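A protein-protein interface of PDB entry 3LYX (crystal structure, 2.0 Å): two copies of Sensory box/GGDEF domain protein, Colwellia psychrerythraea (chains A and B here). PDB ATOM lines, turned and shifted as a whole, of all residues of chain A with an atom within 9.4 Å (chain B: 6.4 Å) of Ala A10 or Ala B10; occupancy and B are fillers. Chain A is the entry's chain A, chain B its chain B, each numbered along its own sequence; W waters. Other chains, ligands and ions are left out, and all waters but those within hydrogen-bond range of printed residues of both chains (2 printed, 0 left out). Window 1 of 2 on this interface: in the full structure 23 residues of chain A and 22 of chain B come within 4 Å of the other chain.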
ATOM      1  N   ASP A   4      18.235  -7.701  -3.733  1.00  0.00           N
ATOM      2  CA  ASP A   4      18.134  -7.232  -2.315  1.00  0.00           C
ATOM      3  C   ASP A   4      17.245  -5.996  -2.235  1.00  0.00           C
ATOM      4  O   ASP A   4      16.035  -6.115  -2.055  1.00  0.00           O
ATOM      5  CB  ASP A   4      19.524  -6.914  -1.771  1.00  0.00           C
ATOM      6  CG  ASP A   4      19.487  -6.339  -0.370  1.00  0.00           C
ATOM      7  OD1 ASP A   4      19.820  -5.146  -0.202  1.00  0.00           O
ATOM      8  OD2 ASP A   4      19.126  -7.077   0.565  1.00  0.00           O
ATOM      9  N   ILE A   5      17.842  -4.814  -2.362  1.00  0.00           N
ATOM     10  CA  ILE A   5      17.079  -3.567  -2.333  1.00  0.00           C
ATOM     11  C   ILE A   5      16.009  -3.651  -3.414  1.00  0.00           C
ATOM     12  O   ILE A   5      14.847  -3.302  -3.201  1.00  0.00           O
ATOM     13  CB  ILE A   5      17.974  -2.350  -2.654  1.00  0.00           C
ATOM     14  CG1 ILE A   5      18.835  -1.992  -1.444  1.00  0.00           C
ATOM     15  CG2 ILE A   5      17.112  -1.164  -3.088  1.00  0.00           C
ATOM     16  CD1 ILE A   5      19.728  -0.781  -1.674  1.00  0.00           C
ATOM     17  N   LEU A   6      16.425  -4.114  -4.585  1.00  0.00           N
ATOM     18  CA  LEU A   6      15.529  -4.252  -5.717  1.00  0.00           C
ATOM     19  C   LEU A   6      14.491  -5.319  -5.403  1.00  0.00           C
ATOM     20  O   LEU A   6      13.300  -5.154  -5.682  1.00  0.00           O
ATOM     21  CB  LEU A   6      16.326  -4.661  -6.952  1.00  0.00           C
ATOM     22  CG  LEU A   6      15.651  -4.514  -8.312  1.00  0.00           C
ATOM     23  CD1 LEU A   6      15.332  -3.039  -8.579  1.00  0.00           C
ATOM     24  CD2 LEU A   6      16.584  -5.066  -9.389  1.00  0.00           C
ATOM     25  N   LYS A   7      14.944  -6.414  -4.807  1.00  0.00           N
ATOM     26  CA  LYS A   7      14.035  -7.499  -4.475  1.00  0.00           C
ATOM     27  C   LYS A   7      12.902  -7.017  -3.572  1.00  0.00           C
ATOM     28  O   LYS A   7      11.732  -7.309  -3.829  1.00  0.00           O
ATOM     29  CB  LYS A   7      14.800  -8.640  -3.801  1.00  0.00           C
ATOM     30  CG  LYS A   7      14.029  -9.958  -3.738  1.00  0.00           C
ATOM     31  CD  LYS A   7      14.902 -11.094  -3.204  1.00  0.00           C
ATOM     32  CE  LYS A   7      14.199 -12.451  -3.316  1.00  0.00           C
ATOM     33  NZ  LYS A   7      15.038 -13.583  -2.806  1.00  0.00           N
ATOM     34  N   GLN A   8      13.242  -6.252  -2.534  1.00  0.00           N
ATOM     35  CA  GLN A   8      12.233  -5.775  -1.597  1.00  0.00           C
ATOM     36  C   GLN A   8      11.250  -4.800  -2.221  1.00  0.00           C
ATOM     37  O   GLN A   8      10.059  -4.820  -1.903  1.00  0.00           O
ATOM     38  CB  GLN A   8      12.900  -5.147  -0.368  1.00  0.00           C
ATOM     39  CG  GLN A   8      13.970  -6.036   0.268  1.00  0.00           C
ATOM     40  CD  GLN A   8      13.490  -7.453   0.561  1.00  0.00           C
ATOM     41  OE1 GLN A   8      14.271  -8.305   0.991  1.00  0.00           O
ATOM     42  NE2 GLN A   8      12.210  -7.709   0.334  1.00  0.00           N
ATOM     43  N   ARG A   9      11.736  -3.945  -3.113  1.00  0.00           N
ATOM     44  CA  ARG A   9      10.839  -3.003  -3.769  1.00  0.00           C
ATOM     45  C   ARG A   9       9.830  -3.788  -4.598  1.00  0.00           C
ATOM     46  O   ARG A   9       8.652  -3.438  -4.652  1.00  0.00           O
ATOM     47  CB  ARG A   9      11.620  -2.061  -4.680  1.00  0.00           C
ATOM     48  CG  ARG A   9      12.232  -0.879  -3.967  1.00  0.00           C
ATOM     49  CD  ARG A   9      13.165  -0.148  -4.905  1.00  0.00           C
ATOM     50  NE  ARG A   9      13.569   1.147  -4.376  1.00  0.00           N
ATOM     51  CZ  ARG A   9      14.638   1.818  -4.791  1.00  0.00           C
ATOM     52  NH1 ARG A   9      15.418   1.314  -5.740  1.00  0.00           N
ATOM     53  NH2 ARG A   9      14.926   2.996  -4.259  1.00  0.00           N
ATOM     54  N   ALA A  10      10.301  -4.855  -5.236  1.00  0.00           N
ATOM     55  CA  ALA A  10       9.445  -5.692  -6.073  1.00  0.00           C
ATOM     56  C   ALA A  10       8.433  -6.516  -5.283  1.00  0.00           C
ATOM     57  O   ALA A  10       7.365  -6.856  -5.792  1.00  0.00           O
ATOM     58  CB  ALA A  10      10.295  -6.605  -6.922  1.00  0.00           C
ATOM     59  N   LYS A  11       8.763  -6.830  -4.034  1.00  0.00           N
ATOM     60  CA  LYS A  11       7.876  -7.625  -3.193  1.00  0.00           C
ATOM     61  C   LYS A  11       6.580  -6.896  -2.865  1.00  0.00           C
ATOM     62  O   LYS A  11       5.533  -7.523  -2.729  1.00  0.00           O
ATOM     63  CB  LYS A  11       8.591  -8.014  -1.890  1.00  0.00           C
ATOM     64  CG  LYS A  11       7.801  -8.989  -1.010  1.00  0.00           C
ATOM     65  CD  LYS A  11       8.498  -9.207   0.331  1.00  0.00           C
ATOM     66  CE  LYS A  11       7.595  -9.935   1.331  1.00  0.00           C
ATOM     67  NZ  LYS A  11       7.352 -11.353   0.961  1.00  0.00           N
ATOM     68  N   ALA A  12       6.641  -5.572  -2.739  1.00  0.00           N
ATOM     69  CA  ALA A  12       5.452  -4.790  -2.419  1.00  0.00           C
ATOM     70  C   ALA A  12       4.353  -4.988  -3.464  1.00  0.00           C
ATOM     71  O   ALA A  12       3.187  -4.687  -3.212  1.00  0.00           O
ATOM     72  CB  ALA A  12       5.813  -3.305  -2.308  1.00  0.00           C
ATOM     73  N   PHE A  13       4.741  -5.515  -4.622  1.00  0.00           N
ATOM     74  CA  PHE A  13       3.841  -5.748  -5.757  1.00  0.00           C
ATOM     75  C   PHE A  13       2.493  -6.371  -5.365  1.00  0.00           C
ATOM     76  O   PHE A  13       1.438  -5.760  -5.557  1.00  0.00           O
ATOM     77  CB  PHE A  13       4.557  -6.643  -6.785  1.00  0.00           C
ATOM     78  CG  PHE A  13       3.970  -6.587  -8.183  1.00  0.00           C
ATOM     79  CD1 PHE A  13       4.009  -5.409  -8.928  1.00  0.00           C
ATOM     80  CD2 PHE A  13       3.421  -7.728  -8.765  1.00  0.00           C
ATOM     81  CE1 PHE A  13       3.515  -5.371 -10.236  1.00  0.00           C
ATOM     82  CE2 PHE A  13       2.921  -7.704 -10.071  1.00  0.00           C
ATOM     83  CZ  PHE A  13       2.970  -6.524 -10.808  1.00  0.00           C
ATOM     84  N   ASP A  14       2.534  -7.577  -4.806  1.00  0.00           N
ATOM     85  CA  ASP A  14       1.314  -8.266  -4.417  1.00  0.00           C
ATOM     86  C   ASP A  14       0.787  -7.949  -3.025  1.00  0.00           C
ATOM     87  O   ASP A  14       0.032  -8.736  -2.462  1.00  0.00           O
ATOM     88  CB  ASP A  14       1.488  -9.783  -4.559  1.00  0.00           C
ATOM     89  CG  ASP A  14       1.413 -10.244  -6.000  1.00  0.00           C
ATOM     90  OD1 ASP A  14       0.615  -9.656  -6.762  1.00  0.00           O
ATOM     91  OD2 ASP A  14       2.140 -11.198  -6.367  1.00  0.00           O
ATOM     92  N   TYR A  15       1.166  -6.800  -2.474  1.00  0.00           N
ATOM     93  CA  TYR A  15       0.692  -6.418  -1.149  1.00  0.00           C
ATOM     94  C   TYR A  15      -0.021  -5.065  -1.184  1.00  0.00           C
ATOM     95  O   TYR A  15      -0.898  -4.796  -0.365  1.00  0.00           O
ATOM     96  CB  TYR A  15       1.865  -6.379  -0.158  1.00  0.00           C
ATOM     97  CG  TYR A  15       2.389  -7.748   0.226  1.00  0.00           C
ATOM     98  CD1 TYR A  15       1.701  -8.554   1.145  1.00  0.00           C
ATOM     99  CD2 TYR A  15       3.554  -8.252  -0.345  1.00  0.00           C
ATOM    100  CE1 TYR A  15       2.175  -9.833   1.479  1.00  0.00           C
ATOM    101  CE2 TYR A  15       4.029  -9.519  -0.022  1.00  0.00           C
ATOM    102  CZ  TYR A  15       3.336 -10.302   0.889  1.00  0.00           C
ATOM    103  OH  TYR A  15       3.813 -11.553   1.197  1.00  0.00           O
ATOM    104  N   VAL A  16       0.328  -4.221  -2.148  1.00  0.00           N
ATOM    105  CA  VAL A  16      -0.310  -2.908  -2.241  1.00  0.00           C
ATOM    106  C   VAL A  16      -1.776  -2.991  -2.654  1.00  0.00           C
ATOM    107  O   VAL A  16      -2.201  -3.962  -3.284  1.00  0.00           O
ATOM    108  CB  VAL A  16       0.431  -1.989  -3.244  1.00  0.00           C
ATOM    109  CG1 VAL A  16       1.843  -1.725  -2.750  1.00  0.00           C
ATOM    110  CG2 VAL A  16       0.462  -2.643  -4.626  1.00  0.00           C
ATOM    111  N   ILE A  20      -1.857  -2.748 -10.169  1.00  0.00           N
ATOM    112  CA  ILE A  20      -0.747  -2.558 -11.106  1.00  0.00           C
ATOM    113  C   ILE A  20      -0.898  -3.415 -12.358  1.00  0.00           C
ATOM    114  O   ILE A  20      -1.043  -4.635 -12.273  1.00  0.00           O
ATOM    115  CB  ILE A  20       0.608  -2.939 -10.464  1.00  0.00           C
ATOM    116  CG1 ILE A  20       0.805  -2.183  -9.140  1.00  0.00           C
ATOM    117  CG2 ILE A  20       1.738  -2.671 -11.456  1.00  0.00           C
ATOM    118  CD1 ILE A  20       0.985  -0.698  -9.295  1.00  0.00           C
ATOM    119  N   VAL A  22       1.042  -4.164 -15.961  1.00  0.00           N
ATOM    120  CA  VAL A  22       2.232  -3.955 -16.765  1.00  0.00           C
ATOM    121  C   VAL A  22       1.974  -4.423 -18.198  1.00  0.00           C
ATOM    122  O   VAL A  22       1.513  -5.543 -18.421  1.00  0.00           O
ATOM    123  CB  VAL A  22       3.438  -4.718 -16.186  1.00  0.00           C
ATOM    124  CG1 VAL A  22       4.676  -4.383 -16.979  1.00  0.00           C
ATOM    125  CG2 VAL A  22       3.638  -4.350 -14.706  1.00  0.00           C
ATOM    126  N   ASP A  31       2.283  -8.361 -16.934  1.00  0.00           N
ATOM    127  CA  ASP A  31       2.367  -8.573 -15.491  1.00  0.00           C
ATOM    128  C   ASP A  31       1.090  -8.028 -14.871  1.00  0.00           C
ATOM    129  O   ASP A  31       0.483  -7.083 -15.387  1.00  0.00           O
ATOM    130  CB  ASP A  31       3.605  -7.918 -14.867  1.00  0.00           C
ATOM    131  CG  ASP A  31       4.159  -8.735 -13.690  1.00  0.00           C
ATOM    132  OD1 ASP A  31       3.429  -9.618 -13.184  1.00  0.00           O
ATOM    133  OD2 ASP A  31       5.312  -8.500 -13.267  1.00  0.00           O
ATOM    134  N   ASN A  33      -0.801  -7.694 -10.732  1.00  0.00           N
ATOM    135  CA  ASN A  33      -0.670  -7.900  -9.283  1.00  0.00           C
ATOM    136  C   ASN A  33      -2.002  -8.220  -8.600  1.00  0.00           C
ATOM    137  O   ASN A  33      -3.060  -8.190  -9.233  1.00  0.00           O
ATOM    138  CB  ASN A  33      -0.008  -6.673  -8.614  1.00  0.00           C
ATOM    139  CG  ASN A  33      -0.961  -5.497  -8.442  1.00  0.00           C
ATOM    140  OD1 ASN A  33      -1.916  -5.346  -9.199  1.00  0.00           O
ATOM    141  ND2 ASN A  33      -0.683  -4.639  -7.453  1.00  0.00           N
ATOM    142  N   ILE A 101       8.000   2.536 -19.597  1.00  0.00           N
ATOM    143  CA  ILE A 101       9.139   1.785 -19.097  1.00  0.00           C
ATOM    144  C   ILE A 101      10.148   1.898 -20.230  1.00  0.00           C
ATOM    145  O   ILE A 101       9.788   1.729 -21.396  1.00  0.00           O
ATOM    146  CB  ILE A 101       8.781   0.304 -18.870  1.00  0.00           C
ATOM    147  CG1 ILE A 101       7.668   0.203 -17.821  1.00  0.00           C
ATOM    148  CG2 ILE A 101      10.016  -0.479 -18.419  1.00  0.00           C
ATOM    149  CD1 ILE A 101       7.155  -1.207 -17.596  1.00  0.00           C
ATOM    150  N   LEU A 112       3.709   1.024 -17.574  1.00  0.00           N
ATOM    151  CA  LEU A 112       3.265   0.627 -16.251  1.00  0.00           C
ATOM    152  C   LEU A 112       1.989   1.395 -15.941  1.00  0.00           C
ATOM    153  O   LEU A 112       1.951   2.621 -16.062  1.00  0.00           O
ATOM    154  CB  LEU A 112       4.348   0.975 -15.222  1.00  0.00           C
ATOM    155  CG  LEU A 112       4.035   0.779 -13.740  1.00  0.00           C
ATOM    156  CD1 LEU A 112       3.884  -0.693 -13.455  1.00  0.00           C
ATOM    157  CD2 LEU A 112       5.148   1.376 -12.897  1.00  0.00           C
ATOM    158  N   ILE B   5      11.590  -8.974 -14.751  1.00  0.00           N
ATOM    159  CA  ILE B   5      10.377  -9.020 -13.940  1.00  0.00           C
ATOM    160  C   ILE B   5      10.554  -8.169 -12.681  1.00  0.00           C
ATOM    161  O   ILE B   5       9.697  -7.349 -12.348  1.00  0.00           O
ATOM    162  CB  ILE B   5      10.036 -10.471 -13.501  1.00  0.00           C
ATOM    163  CG1 ILE B   5       9.643 -11.317 -14.716  1.00  0.00           C
ATOM    164  CG2 ILE B   5       8.911 -10.455 -12.470  1.00  0.00           C
ATOM    165  CD1 ILE B   5      10.815 -11.802 -15.555  1.00  0.00           C
ATOM    166  N   LEU B   6      11.669  -8.367 -11.985  1.00  0.00           N
ATOM    167  CA  LEU B   6      11.942  -7.615 -10.763  1.00  0.00           C
ATOM    168  C   LEU B   6      11.999  -6.119 -11.010  1.00  0.00           C
ATOM    169  O   LEU B   6      11.504  -5.330 -10.202  1.00  0.00           O
ATOM    170  CB  LEU B   6      13.266  -8.047 -10.133  1.00  0.00           C
ATOM    171  CG  LEU B   6      13.342  -9.377  -9.389  1.00  0.00           C
ATOM    172  CD1 LEU B   6      14.696  -9.461  -8.688  1.00  0.00           C
ATOM    173  CD2 LEU B   6      12.209  -9.481  -8.369  1.00  0.00           C
ATOM    174  N   LYS B   7      12.617  -5.733 -12.122  1.00  0.00           N
ATOM    175  CA  LYS B   7      12.744  -4.326 -12.466  1.00  0.00           C
ATOM    176  C   LYS B   7      11.383  -3.666 -12.622  1.00  0.00           C
ATOM    177  O   LYS B   7      11.113  -2.638 -12.000  1.00  0.00           O
ATOM    178  CB  LYS B   7      13.546  -4.163 -13.763  1.00  0.00           C
ATOM    179  CG  LYS B   7      15.004  -4.596 -13.648  1.00  0.00           C
ATOM    180  CD  LYS B   7      15.781  -3.732 -12.655  1.00  0.00           C
ATOM    181  CE  LYS B   7      16.003  -2.318 -13.183  1.00  0.00           C
ATOM    182  NZ  LYS B   7      16.869  -1.508 -12.276  1.00  0.00           N
ATOM    183  N   GLN B   8      10.521  -4.264 -13.440  1.00  0.00           N
ATOM    184  CA  GLN B   8       9.203  -3.694 -13.676  1.00  0.00           C
ATOM    185  C   GLN B   8       8.341  -3.657 -12.430  1.00  0.00           C
ATOM    186  O   GLN B   8       7.546  -2.731 -12.250  1.00  0.00           O
ATOM    187  CB  GLN B   8       8.474  -4.452 -14.789  1.00  0.00           C
ATOM    188  CG  GLN B   8       8.268  -5.930 -14.540  1.00  0.00           C
ATOM    189  CD  GLN B   8       7.682  -6.633 -15.755  1.00  0.00           C
ATOM    190  OE1 GLN B   8       8.116  -6.404 -16.886  1.00  0.00           O
ATOM    191  NE2 GLN B   8       6.703  -7.500 -15.526  1.00  0.00           N
ATOM    192  N   ARG B   9       8.497  -4.652 -11.564  1.00  0.00           N
ATOM    193  CA  ARG B   9       7.717  -4.687 -10.339  1.00  0.00           C
ATOM    194  C   ARG B   9       8.212  -3.622  -9.371  1.00  0.00           C
ATOM    195  O   ARG B   9       7.421  -2.987  -8.683  1.00  0.00           O
ATOM    196  CB  ARG B   9       7.783  -6.080  -9.702  1.00  0.00           C
ATOM    197  CG  ARG B   9       7.083  -7.145 -10.535  1.00  0.00           C
ATOM    198  CD  ARG B   9       6.783  -8.393  -9.730  1.00  0.00           C
ATOM    199  NE  ARG B   9       5.836  -9.250 -10.433  1.00  0.00           N
ATOM    200  CZ  ARG B   9       5.180 -10.263  -9.874  1.00  0.00           C
ATOM    201  NH1 ARG B   9       5.367 -10.561  -8.592  1.00  0.00           N
ATOM    202  NH2 ARG B   9       4.317 -10.965 -10.594  1.00  0.00           N
ATOM    203  N   ALA B  10       9.527  -3.423  -9.330  1.00  0.00           N
ATOM    204  CA  ALA B  10      10.115  -2.417  -8.451  1.00  0.00           C
ATOM    205  C   ALA B  10       9.742  -1.026  -8.964  1.00  0.00           C
ATOM    206  O   ALA B  10       9.574  -0.083  -8.188  1.00  0.00           O
ATOM    207  CB  ALA B  10      11.631  -2.579  -8.411  1.00  0.00           C
ATOM    208  N   LYS B  11       9.605  -0.912 -10.279  1.00  0.00           N
ATOM    209  CA  LYS B  11       9.244   0.353 -10.913  1.00  0.00           C
ATOM    210  C   LYS B  11       7.982   0.965 -10.299  1.00  0.00           C
ATOM    211  O   LYS B  11       7.918   2.174 -10.079  1.00  0.00           O
ATOM    212  CB  LYS B  11       9.035   0.127 -12.414  1.00  0.00           C
ATOM    213  CG  LYS B  11       8.473   1.311 -13.186  1.00  0.00           C
ATOM    214  CD  LYS B  11       9.519   2.374 -13.453  1.00  0.00           C
ATOM    215  CE  LYS B  11       9.011   3.361 -14.499  1.00  0.00           C
ATOM    216  NZ  LYS B  11      10.065   4.308 -14.953  1.00  0.00           N
ATOM    217  N   ALA B  12       6.979   0.133 -10.022  1.00  0.00           N
ATOM    218  CA  ALA B  12       5.727   0.621  -9.446  1.00  0.00           C
ATOM    219  C   ALA B  12       5.927   1.289  -8.085  1.00  0.00           C
ATOM    220  O   ALA B  12       5.125   2.135  -7.667  1.00  0.00           O
ATOM    221  CB  ALA B  12       4.727  -0.527  -9.320  1.00  0.00           C
ATOM    222  N   PHE B  13       7.000   0.900  -7.404  1.00  0.00           N
ATOM    223  CA  PHE B  13       7.334   1.425  -6.081  1.00  0.00           C
ATOM    224  C   PHE B  13       7.056   2.917  -5.895  1.00  0.00           C
ATOM    225  O   PHE B  13       6.272   3.303  -5.029  1.00  0.00           O
ATOM    226  CB  PHE B  13       8.807   1.144  -5.778  1.00  0.00           C
ATOM    227  CG  PHE B  13       9.208   1.433  -4.359  1.00  0.00           C
ATOM    228  CD1 PHE B  13       8.750   0.634  -3.318  1.00  0.00           C
ATOM    229  CD2 PHE B  13      10.083   2.478  -4.068  1.00  0.00           C
ATOM    230  CE1 PHE B  13       9.160   0.865  -2.008  1.00  0.00           C
ATOM    231  CE2 PHE B  13      10.501   2.718  -2.759  1.00  0.00           C
ATOM    232  CZ  PHE B  13      10.038   1.910  -1.728  1.00  0.00           C
ATOM    233  N   ASP B  14       7.689   3.767  -6.695  1.00  0.00           N
ATOM    234  CA  ASP B  14       7.461   5.200  -6.538  1.00  0.00           C
ATOM    235  C   ASP B  14       6.259   5.774  -7.277  1.00  0.00           C
ATOM    236  O   ASP B  14       6.122   6.992  -7.372  1.00  0.00           O
ATOM    237  CB  ASP B  14       8.716   6.001  -6.907  1.00  0.00           C
ATOM    238  CG  ASP B  14       9.699   6.113  -5.743  1.00  0.00           C
ATOM    239  OD1 ASP B  14       9.245   6.352  -4.603  1.00  0.00           O
ATOM    240  OD2 ASP B  14      10.920   5.970  -5.968  1.00  0.00           O
HETATM  241  O   HOH W   1       2.793 -12.649  -9.171  1.00  0.00           O
HETATM  242  O   HOH W   2       6.721  -9.590  -6.370  1.00  0.00           O
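OD2 of Asp A14 lies within salt-bridge range of NH1 of Arg B9, at 3.97 Å.
The side-chain amide nitrogen (NE2) of Gln B8 sits at hydrogen-bond distance from the side-chain carboxylate (OD2) of Asp A31, at 2.8 Å.
The side-chain carboxylate (OD2) of Asp A31 lies within salt-bridge range of the guanidinium group (NE) of Arg B9 (3.0 Å).
The backbone NH (N) of Ile A20 lies within hydrogen-bond range of the side-chain amide oxygen (OD1) of Asn A33 (2.8 Å).
The backbone NH of Val A22 lies within hydrogen-bond range of the backbone carbonyl oxygen of Asp A31, at 3.0 Å.
The backbone carbonyl oxygen (O) of Phe A13 is in hydrogen-bond range of the side-chain amide nitrogen (ND2) of Asn A33 (3.1 Å).
Among the printed residues, pairs that only touch across the chains: Leu A6 with Lys B7 (3.6 Å), Leu A6 with Ala B10 (3.7 Å), Arg A9 with Ala B10 (3.8 Å), Arg A9 with Phe B13 (3.7 Å), Ala A10 with Leu B6 (3.7 Å), Ala A10 with Arg B9 (3.8 Å), Ala A10 with Ala B10 (3.97 Å), Phe A13 with Arg B9 (3.3 Å), Ile A20 with Ala B12 (3.7 Å), Val A22 with Gln B8 (3.9 Å), Leu A112 with Lys B11 (3.3 Å) and Leu A112 with Ala B12 (3.6 Å).
Ala B10 touches just these residues of chain A: Leu A6 (3.7 Å), Arg A9 (3.8 Å) and Ala A10 (3.97 Å).
Printed residues of chain A within 4 Å of Arg B9: Ala A10 (3.8 Å), Phe A13 (3.3 Å), Asp A14 (3.97 Å) and Asp A31 (3.0 Å).
Of the printed residues of chain B, Leu A6 touches Lys B7 (3.6 Å) and Ala B10 (3.7 Å).
Printed residues of chain A within 4 Å of Leu B6: Ala A10 (3.7 Å).
Of the printed residues of chain B, Asp A14 touches Arg B9.
Of the printed residues of chain B, Asp A31 touches Gln B8 (2.8 Å) and Arg B9 (3.0 Å).
Gln A8 touches none of the printed residues of chain B.
Asp B14 touches none of the printed residues of chain A.
The nearest residue of chain A that does not touch Ala B10 is Phe A13 (5.9 Å).
The nearest printed residue of chain A that does not touch Leu B6 is Leu A6 (4.5 Å).
Printed residues of chain A that touch a printed residue of chain B: Leu A6, Arg A9, Ala A10, Phe A13, Asp A14, Ile A20, Val A22, Asp A31 and Leu A112.
Hydrophobic or aromatic side chains of chain A that line the printed part of chain B: Leu A6, Ala A10, Phe A13, Ile A20, Val A22 and Leu A112.
Of the 10 printed residues of chain B, 8 touch a printed residue of chain A.
Among the printed residues, 15 pairs touch across the chains.
Among the printed residues, Asp or Glu carboxylates within 4 Å of a Lys or Arg side-chain nitrogen of the other chain: Asp A14 with Arg B9 and Asp A31 with Arg B9.
Leu A6 touches Ala B10, and with the chains exchanged Ala A10 touches Leu B6.
Arg A9 touches Ala B10, and with the chains exchanged Ala A10 touches Arg B9.
Arg A9 touches Phe B13, and with the chains exchanged Phe A13 touches Arg B9.
Asp A14 touches Arg B9, but with the chains exchanged Arg A9 does not touch Asp B14 (5.3 Å).
10 positions are printed for both chains.
Of the 15 pairs that touch across the chains among the printed residues, 7 have their exchanged pair printed and touching as well.
Water W1 lies within hydrogen-bond range of NH2 of Arg B9 and OD2 of Asp A14.
Water W2 bridges the guanidinium group of Arg B9 (2.8 Å) and the backbone carbonyl oxygen of Ala A10 (2.9 Å).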
